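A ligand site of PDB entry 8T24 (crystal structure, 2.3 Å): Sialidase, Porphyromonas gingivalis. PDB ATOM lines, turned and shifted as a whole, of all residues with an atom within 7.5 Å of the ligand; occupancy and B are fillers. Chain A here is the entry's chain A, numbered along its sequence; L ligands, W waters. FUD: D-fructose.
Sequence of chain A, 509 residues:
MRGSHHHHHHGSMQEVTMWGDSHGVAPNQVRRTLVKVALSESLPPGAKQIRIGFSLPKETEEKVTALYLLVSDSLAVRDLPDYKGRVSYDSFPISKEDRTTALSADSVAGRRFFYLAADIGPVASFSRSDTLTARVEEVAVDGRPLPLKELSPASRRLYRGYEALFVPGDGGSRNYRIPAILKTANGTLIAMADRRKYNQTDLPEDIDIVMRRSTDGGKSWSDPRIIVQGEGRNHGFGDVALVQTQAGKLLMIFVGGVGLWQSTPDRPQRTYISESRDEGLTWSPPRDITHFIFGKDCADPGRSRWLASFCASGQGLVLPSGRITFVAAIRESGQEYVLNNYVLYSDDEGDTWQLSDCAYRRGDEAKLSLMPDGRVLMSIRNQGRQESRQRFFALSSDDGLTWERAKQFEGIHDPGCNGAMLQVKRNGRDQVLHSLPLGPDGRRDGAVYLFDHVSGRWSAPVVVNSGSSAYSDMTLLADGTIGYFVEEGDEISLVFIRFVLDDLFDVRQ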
ATOM      1  N   TRP A  19       8.834 -31.580  37.426  1.00  0.00           N
ATOM      2  CA  TRP A  19       9.853 -31.597  36.378  1.00  0.00           C
ATOM      3  C   TRP A  19      11.244 -31.689  36.997  1.00  0.00           C
ATOM      4  O   TRP A  19      11.669 -30.765  37.704  1.00  0.00           O
ATOM      5  CB  TRP A  19       9.768 -30.346  35.500  1.00  0.00           C
ATOM      6  CG  TRP A  19       8.453 -30.116  34.816  1.00  0.00           C
ATOM      7  CD1 TRP A  19       8.154 -30.397  33.513  1.00  0.00           C
ATOM      8  CD2 TRP A  19       7.270 -29.540  35.393  1.00  0.00           C
ATOM      9  NE1 TRP A  19       6.850 -30.035  33.238  1.00  0.00           N
ATOM     10  CE2 TRP A  19       6.291 -29.503  34.377  1.00  0.00           C
ATOM     11  CE3 TRP A  19       6.946 -29.054  36.661  1.00  0.00           C
ATOM     12  CZ2 TRP A  19       5.006 -28.995  34.597  1.00  0.00           C
ATOM     13  CZ3 TRP A  19       5.676 -28.548  36.877  1.00  0.00           C
ATOM     14  CH2 TRP A  19       4.721 -28.518  35.846  1.00  0.00           C
ATOM     15  N   GLY A  20      11.958 -32.773  36.732  1.00  0.00           N
ATOM     16  CA  GLY A  20      13.372 -32.794  37.031  1.00  0.00           C
ATOM     17  C   GLY A  20      14.157 -31.944  36.052  1.00  0.00           C
ATOM     18  O   GLY A  20      13.773 -31.785  34.888  1.00  0.00           O
ATOM     19  N   ASP A  21      15.259 -31.361  36.520  1.00  0.00           N
ATOM     20  CA  ASP A  21      16.094 -30.555  35.633  1.00  0.00           C
ATOM     21  C   ASP A  21      17.112 -31.449  34.928  1.00  0.00           C
ATOM     22  O   ASP A  21      17.677 -32.361  35.538  1.00  0.00           O
ATOM     23  CB  ASP A  21      16.849 -29.465  36.392  1.00  0.00           C
ATOM     24  CG  ASP A  21      17.395 -28.387  35.457  1.00  0.00           C
ATOM     25  OD1 ASP A  21      18.442 -28.636  34.813  1.00  0.00           O
ATOM     26  OD2 ASP A  21      16.851 -27.243  35.458  1.00  0.00           O
ATOM     27  N   SER A  22      17.368 -31.160  33.644  1.00  0.00           N
ATOM     28  CA  SER A  22      18.363 -31.878  32.849  1.00  0.00           C
ATOM     29  C   SER A  22      19.463 -30.965  32.316  1.00  0.00           C
ATOM     30  O   SER A  22      20.219 -31.383  31.432  1.00  0.00           O
ATOM     31  CB  SER A  22      17.708 -32.596  31.651  1.00  0.00           C
ATOM     32  OG  SER A  22      16.423 -33.076  31.979  1.00  0.00           O
ATOM     33  N   HIS A  23      19.577 -29.743  32.802  1.00  0.00           N
ATOM     34  CA  HIS A  23      20.591 -28.831  32.274  1.00  0.00           C
ATOM     35  C   HIS A  23      21.937 -29.108  32.927  1.00  0.00           C
ATOM     36  O   HIS A  23      22.024 -29.614  34.056  1.00  0.00           O
ATOM     37  CB  HIS A  23      20.182 -27.376  32.511  1.00  0.00           C
ATOM     38  CG  HIS A  23      19.005 -26.948  31.674  1.00  0.00           C
ATOM     39  ND1 HIS A  23      17.954 -26.231  32.202  1.00  0.00           N
ATOM     40  CD2 HIS A  23      18.729 -27.132  30.369  1.00  0.00           C
ATOM     41  CE1 HIS A  23      17.074 -25.989  31.244  1.00  0.00           C
ATOM     42  NE2 HIS A  23      17.520 -26.521  30.117  1.00  0.00           N
ATOM     43  N   VAL A  77      11.704 -22.122  33.387  1.00  0.00           N
ATOM     44  CA  VAL A  77      12.397 -23.194  32.682  1.00  0.00           C
ATOM     45  C   VAL A  77      13.774 -23.418  33.295  1.00  0.00           C
ATOM     46  O   VAL A  77      14.140 -24.554  33.642  1.00  0.00           O
ATOM     47  CB  VAL A  77      12.475 -22.862  31.181  1.00  0.00           C
ATOM     48  CG1 VAL A  77      13.530 -23.718  30.468  1.00  0.00           C
ATOM     49  CG2 VAL A  77      11.123 -23.046  30.524  1.00  0.00           C
ATOM     50  N   ARG A  78      14.551 -22.351  33.455  1.00  0.00           N
ATOM     51  CA  ARG A  78      15.940 -22.433  33.868  1.00  0.00           C
ATOM     52  C   ARG A  78      16.104 -22.149  35.355  1.00  0.00           C
ATOM     53  O   ARG A  78      15.162 -21.765  36.045  1.00  0.00           O
ATOM     54  CB  ARG A  78      16.785 -21.454  33.048  1.00  0.00           C
ATOM     55  CG  ARG A  78      16.654 -21.635  31.541  1.00  0.00           C
ATOM     56  CD  ARG A  78      17.850 -21.078  30.796  1.00  0.00           C
ATOM     57  NE  ARG A  78      19.101 -21.699  31.207  1.00  0.00           N
ATOM     58  CZ  ARG A  78      19.611 -22.791  30.677  1.00  0.00           C
ATOM     59  NH1 ARG A  78      19.038 -23.401  29.642  1.00  0.00           N
ATOM     60  NH2 ARG A  78      20.734 -23.307  31.177  1.00  0.00           N
ATOM     61  N   LEU A 151       6.533 -35.377  34.918  1.00  0.00           N
ATOM     62  CA  LEU A 151       6.646 -35.109  33.489  1.00  0.00           C
ATOM     63  C   LEU A 151       8.086 -35.179  32.990  1.00  0.00           C
ATOM     64  O   LEU A 151       8.293 -35.248  31.777  1.00  0.00           O
ATOM     65  CB  LEU A 151       6.081 -33.724  33.162  1.00  0.00           C
ATOM     66  CG  LEU A 151       4.568 -33.549  33.295  1.00  0.00           C
ATOM     67  CD1 LEU A 151       4.220 -32.082  33.233  1.00  0.00           C
ATOM     68  CD2 LEU A 151       3.840 -34.313  32.228  1.00  0.00           C
ATOM     69  N   SER A 152       9.069 -35.152  33.886  1.00  0.00           N
ATOM     70  CA  SER A 152      10.476 -35.114  33.503  1.00  0.00           C
ATOM     71  C   SER A 152      11.363 -35.653  34.611  1.00  0.00           C
ATOM     72  O   SER A 152      11.138 -35.320  35.779  1.00  0.00           O
ATOM     73  CB  SER A 152      10.895 -33.685  33.161  1.00  0.00           C
ATOM     74  OG  SER A 152      12.166 -33.710  32.536  1.00  0.00           O
ATOM     75  N   PRO A 153      12.381 -36.433  34.283  1.00  0.00           N
ATOM     76  CA  PRO A 153      13.346 -36.866  35.296  1.00  0.00           C
ATOM     77  C   PRO A 153      14.538 -35.918  35.344  1.00  0.00           C
ATOM     78  O   PRO A 153      14.803 -35.163  34.404  1.00  0.00           O
ATOM     79  CB  PRO A 153      13.754 -38.261  34.812  1.00  0.00           C
ATOM     80  CG  PRO A 153      13.725 -38.102  33.299  1.00  0.00           C
ATOM     81  CD  PRO A 153      12.666 -37.057  32.972  1.00  0.00           C
ATOM     82  N   ARG A 443      14.932 -31.592  16.678  1.00  0.00           N
ATOM     83  CA  ARG A 443      15.930 -30.741  17.327  1.00  0.00           C
ATOM     84  C   ARG A 443      16.077 -31.108  18.800  1.00  0.00           C
ATOM     85  O   ARG A 443      15.634 -30.415  19.718  1.00  0.00           O
ATOM     86  CB  ARG A 443      15.554 -29.275  17.133  1.00  0.00           C
ATOM     87  CG  ARG A 443      15.412 -28.886  15.670  1.00  0.00           C
ATOM     88  CD  ARG A 443      16.606 -28.095  15.199  1.00  0.00           C
ATOM     89  NE  ARG A 443      16.581 -27.811  13.769  1.00  0.00           N
ATOM     90  CZ  ARG A 443      16.438 -26.600  13.240  1.00  0.00           C
ATOM     91  NH1 ARG A 443      16.245 -25.534  14.003  1.00  0.00           N
ATOM     92  NH2 ARG A 443      16.490 -26.460  11.924  1.00  0.00           N
ATOM     93  N   ARG A 444      16.738 -32.242  19.016  1.00  0.00           N
ATOM     94  CA  ARG A 444      16.854 -32.836  20.339  1.00  0.00           C
ATOM     95  C   ARG A 444      18.268 -33.353  20.582  1.00  0.00           C
ATOM     96  O   ARG A 444      18.951 -33.824  19.666  1.00  0.00           O
ATOM     97  CB  ARG A 444      15.849 -33.980  20.507  1.00  0.00           C
ATOM     98  CG  ARG A 444      14.478 -33.451  20.837  1.00  0.00           C
ATOM     99  CD  ARG A 444      13.703 -34.464  21.631  1.00  0.00           C
ATOM    100  NE  ARG A 444      14.204 -34.645  22.995  1.00  0.00           N
ATOM    101  CZ  ARG A 444      13.790 -33.951  24.047  1.00  0.00           C
ATOM    102  NH1 ARG A 444      12.985 -32.916  23.930  1.00  0.00           N
ATOM    103  NH2 ARG A 444      14.169 -34.337  25.267  1.00  0.00           N
ATOM    104  N   ASP A 445      18.688 -33.246  21.848  1.00  0.00           N
ATOM    105  CA  ASP A 445      19.930 -33.840  22.354  1.00  0.00           C
ATOM    106  C   ASP A 445      21.162 -33.355  21.578  1.00  0.00           C
ATOM    107  O   ASP A 445      21.619 -34.008  20.644  1.00  0.00           O
ATOM    108  CB  ASP A 445      19.847 -35.365  22.334  1.00  0.00           C
ATOM    109  CG  ASP A 445      18.661 -35.899  23.134  1.00  0.00           C
ATOM    110  OD1 ASP A 445      18.221 -35.210  24.090  1.00  0.00           O
ATOM    111  OD2 ASP A 445      18.167 -36.988  22.802  1.00  0.00           O
ATOM    112  N   ASN A 465      24.085 -31.820  25.662  1.00  0.00           N
ATOM    113  CA  ASN A 465      22.921 -31.233  26.334  1.00  0.00           C
ATOM    114  C   ASN A 465      21.667 -31.923  25.831  1.00  0.00           C
ATOM    115  O   ASN A 465      21.295 -31.783  24.662  1.00  0.00           O
ATOM    116  CB  ASN A 465      22.824 -29.719  26.096  1.00  0.00           C
ATOM    117  CG  ASN A 465      22.811 -29.357  24.631  1.00  0.00           C
ATOM    118  OD1 ASN A 465      23.795 -29.569  23.928  1.00  0.00           O
ATOM    119  ND2 ASN A 465      21.684 -28.784  24.149  1.00  0.00           N
ATOM    120  N   SER A 466      21.004 -32.651  26.727  1.00  0.00           N
ATOM    121  CA  SER A 466      19.775 -33.362  26.407  1.00  0.00           C
ATOM    122  C   SER A 466      18.615 -32.371  26.379  1.00  0.00           C
ATOM    123  O   SER A 466      18.682 -31.272  26.924  1.00  0.00           O
ATOM    124  CB  SER A 466      19.507 -34.449  27.448  1.00  0.00           C
ATOM    125  OG  SER A 466      19.309 -33.860  28.714  1.00  0.00           O
ATOM    126  N   GLY A 467      17.527 -32.786  25.743  1.00  0.00           N
ATOM    127  CA  GLY A 467      16.366 -31.940  25.594  1.00  0.00           C
ATOM    128  C   GLY A 467      16.359 -31.235  24.258  1.00  0.00           C
ATOM    129  O   GLY A 467      17.069 -31.608  23.327  1.00  0.00           O
ATOM    130  N   SER A 468      15.539 -30.195  24.167  1.00  0.00           N
ATOM    131  CA  SER A 468      15.496 -29.415  22.943  1.00  0.00           C
ATOM    132  C   SER A 468      16.846 -28.777  22.697  1.00  0.00           C
ATOM    133  O   SER A 468      17.390 -28.088  23.567  1.00  0.00           O
ATOM    134  CB  SER A 468      14.413 -28.337  23.009  1.00  0.00           C
ATOM    135  OG  SER A 468      13.129 -28.910  23.044  1.00  0.00           O
ATOM    136  N   SER A 469      17.396 -29.010  21.502  1.00  0.00           N
ATOM    137  CA  SER A 469      18.708 -28.479  21.150  1.00  0.00           C
ATOM    138  C   SER A 469      18.701 -28.098  19.673  1.00  0.00           C
ATOM    139  O   SER A 469      18.086 -28.803  18.869  1.00  0.00           O
ATOM    140  CB  SER A 469      19.780 -29.526  21.473  1.00  0.00           C
ATOM    141  OG  SER A 469      21.070 -28.993  21.364  1.00  0.00           O
ATOM    142  N   GLU A 488      19.490 -23.914  23.653  1.00  0.00           N
ATOM    143  CA  GLU A 488      18.906 -24.838  24.610  1.00  0.00           C
ATOM    144  C   GLU A 488      17.430 -24.543  24.842  1.00  0.00           C
ATOM    145  O   GLU A 488      17.074 -23.425  25.225  1.00  0.00           O
ATOM    146  CB  GLU A 488      19.630 -24.762  25.952  1.00  0.00           C
ATOM    147  CG  GLU A 488      20.767 -25.735  26.107  1.00  0.00           C
ATOM    148  CD  GLU A 488      21.233 -25.836  27.533  1.00  0.00           C
ATOM    149  OE1 GLU A 488      20.485 -25.379  28.430  1.00  0.00           O
ATOM    150  OE2 GLU A 488      22.331 -26.367  27.753  1.00  0.00           O
ATOM    151  N   GLY A 489      16.585 -25.541  24.653  1.00  0.00           N
ATOM    152  CA  GLY A 489      15.220 -25.462  25.100  1.00  0.00           C
ATOM    153  C   GLY A 489      14.259 -25.123  23.971  1.00  0.00           C
ATOM    154  O   GLY A 489      14.662 -24.821  22.847  1.00  0.00           O
ATOM    155  N   ASP A 490      12.966 -25.220  24.279  1.00  0.00           N
ATOM    156  CA  ASP A 490      11.957 -24.842  23.287  1.00  0.00           C
ATOM    157  C   ASP A 490      11.900 -23.324  23.141  1.00  0.00           C
ATOM    158  O   ASP A 490      11.944 -22.795  22.028  1.00  0.00           O
ATOM    159  CB  ASP A 490      10.584 -25.387  23.666  1.00  0.00           C
ATOM    160  CG  ASP A 490      10.397 -26.830  23.255  1.00  0.00           C
ATOM    161  OD1 ASP A 490      11.115 -27.322  22.340  1.00  0.00           O
ATOM    162  OD2 ASP A 490       9.506 -27.482  23.850  1.00  0.00           O
ATOM    163  N   GLU A 491      11.767 -22.629  24.257  1.00  0.00           N
ATOM    164  CA  GLU A 491      12.064 -21.209  24.314  1.00  0.00           C
ATOM    165  C   GLU A 491      13.553 -21.097  24.600  1.00  0.00           C
ATOM    166  O   GLU A 491      14.010 -21.352  25.711  1.00  0.00           O
ATOM    167  CB  GLU A 491      11.221 -20.519  25.385  1.00  0.00           C
ATOM    168  CG  GLU A 491      11.323 -19.023  25.319  1.00  0.00           C
ATOM    169  CD  GLU A 491       9.972 -18.351  25.208  1.00  0.00           C
ATOM    170  OE1 GLU A 491       9.374 -18.360  24.098  1.00  0.00           O
ATOM    171  OE2 GLU A 491       9.506 -17.814  26.256  1.00  0.00           O
ATOM    172  N   ILE A 492      14.309 -20.740  23.571  1.00  0.00           N
ATOM    173  CA  ILE A 492      15.738 -21.030  23.517  1.00  0.00           C
ATOM    174  C   ILE A 492      16.537 -20.099  24.410  1.00  0.00           C
ATOM    175  O   ILE A 492      16.284 -18.889  24.460  1.00  0.00           O
ATOM    176  CB  ILE A 492      16.201 -20.946  22.055  1.00  0.00           C
ATOM    177  CG1 ILE A 492      15.624 -22.122  21.252  1.00  0.00           C
ATOM    178  CG2 ILE A 492      17.696 -20.808  21.969  1.00  0.00           C
ATOM    179  CD1 ILE A 492      15.916 -22.016  19.773  1.00  0.00           C
ATOM    180  N   SER A 493      17.507 -20.666  25.128  1.00  0.00           N
ATOM    181  CA  SER A 493      18.592 -19.922  25.749  1.00  0.00           C
ATOM    182  C   SER A 493      19.879 -20.248  25.013  1.00  0.00           C
ATOM    183  O   SER A 493      20.059 -21.370  24.521  1.00  0.00           O
ATOM    184  CB  SER A 493      18.736 -20.261  27.230  1.00  0.00           C
ATOM    185  OG  SER A 493      17.790 -19.556  27.994  1.00  0.00           O
HETATM  186  C1  FUD L   1      13.358 -26.019  27.977  1.00  0.00           C
HETATM  187  C2  FUD L   1      12.692 -27.280  27.415  1.00  0.00           C
HETATM  188  C3  FUD L   1      12.792 -28.606  28.152  1.00  0.00           C
HETATM  189  C4  FUD L   1      13.830 -29.550  27.516  1.00  0.00           C
HETATM  190  C5  FUD L   1      13.138 -30.529  26.569  1.00  0.00           C
HETATM  191  C6  FUD L   1      12.783 -31.840  27.276  1.00  0.00           C
HETATM  192  O1  FUD L   1      14.600 -26.301  28.570  1.00  0.00           O
HETATM  193  O2  FUD L   1      12.052 -27.224  26.400  1.00  0.00           O
HETATM  194  O3  FUD L   1      11.524 -29.190  28.058  1.00  0.00           O
HETATM  195  O4  FUD L   1      14.792 -28.848  26.753  1.00  0.00           O
HETATM  196  O5  FUD L   1      12.005 -29.902  26.023  1.00  0.00           O
HETATM  197  O6  FUD L   1      13.881 -32.250  28.033  1.00  0.00           O
HETATM  198  O   HOH W   1      17.129 -28.043  27.288  1.00  0.00           O
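An oxygen (O4) of the ligand sits at hydrogen-bond distance from the backbone NH (N) of Ser 468 (3.0 Å).
O5 of the ligand lies within hydrogen-bond range of OG of Ser 468.
N of Asp 490 lies within hydrogen-bond range of O2 of the ligand (3.1 Å).
NE2 of His 23 lies within hydrogen-bond range of O1 of the ligand (3.3 Å).
An oxygen (O6) of the ligand is in hydrogen-bond range of the guanidinium group of Arg 444 (3.5 Å).
The side-chain hydroxyl of Ser 468 lies within hydrogen-bond range of the side-chain carboxylate of Asp 490, at 2.7 Å.
The backbone NH of Gly 489 sits at hydrogen-bond distance from the backbone carbonyl oxygen of Ser 468, 2.9 Å away.
The backbone NH of His 23 is in hydrogen-bond range of the side-chain carboxylate of Asp 21 (2.6 Å).
N of Asp 445 is in hydrogen-bond range of O of Gly 467.
Residues that only touch the ligand: Val 77 (3.4 Å), Gly 489 (3.5 Å) and Gly 467 (3.5 Å).
Hydrophobic or aromatic side chains that line the ligand: His 23 and Val 77.
Of the 24 residues printed, 7 come within 4 Å of the ligand.
The nearest printed residue that does not touch the ligand is Ser 466 (4.6 Å).
Water W1 bridges an oxygen (O4) of the ligand (2.5 Å) and a ring nitrogen (NE2) of His 23 (3.2 Å).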
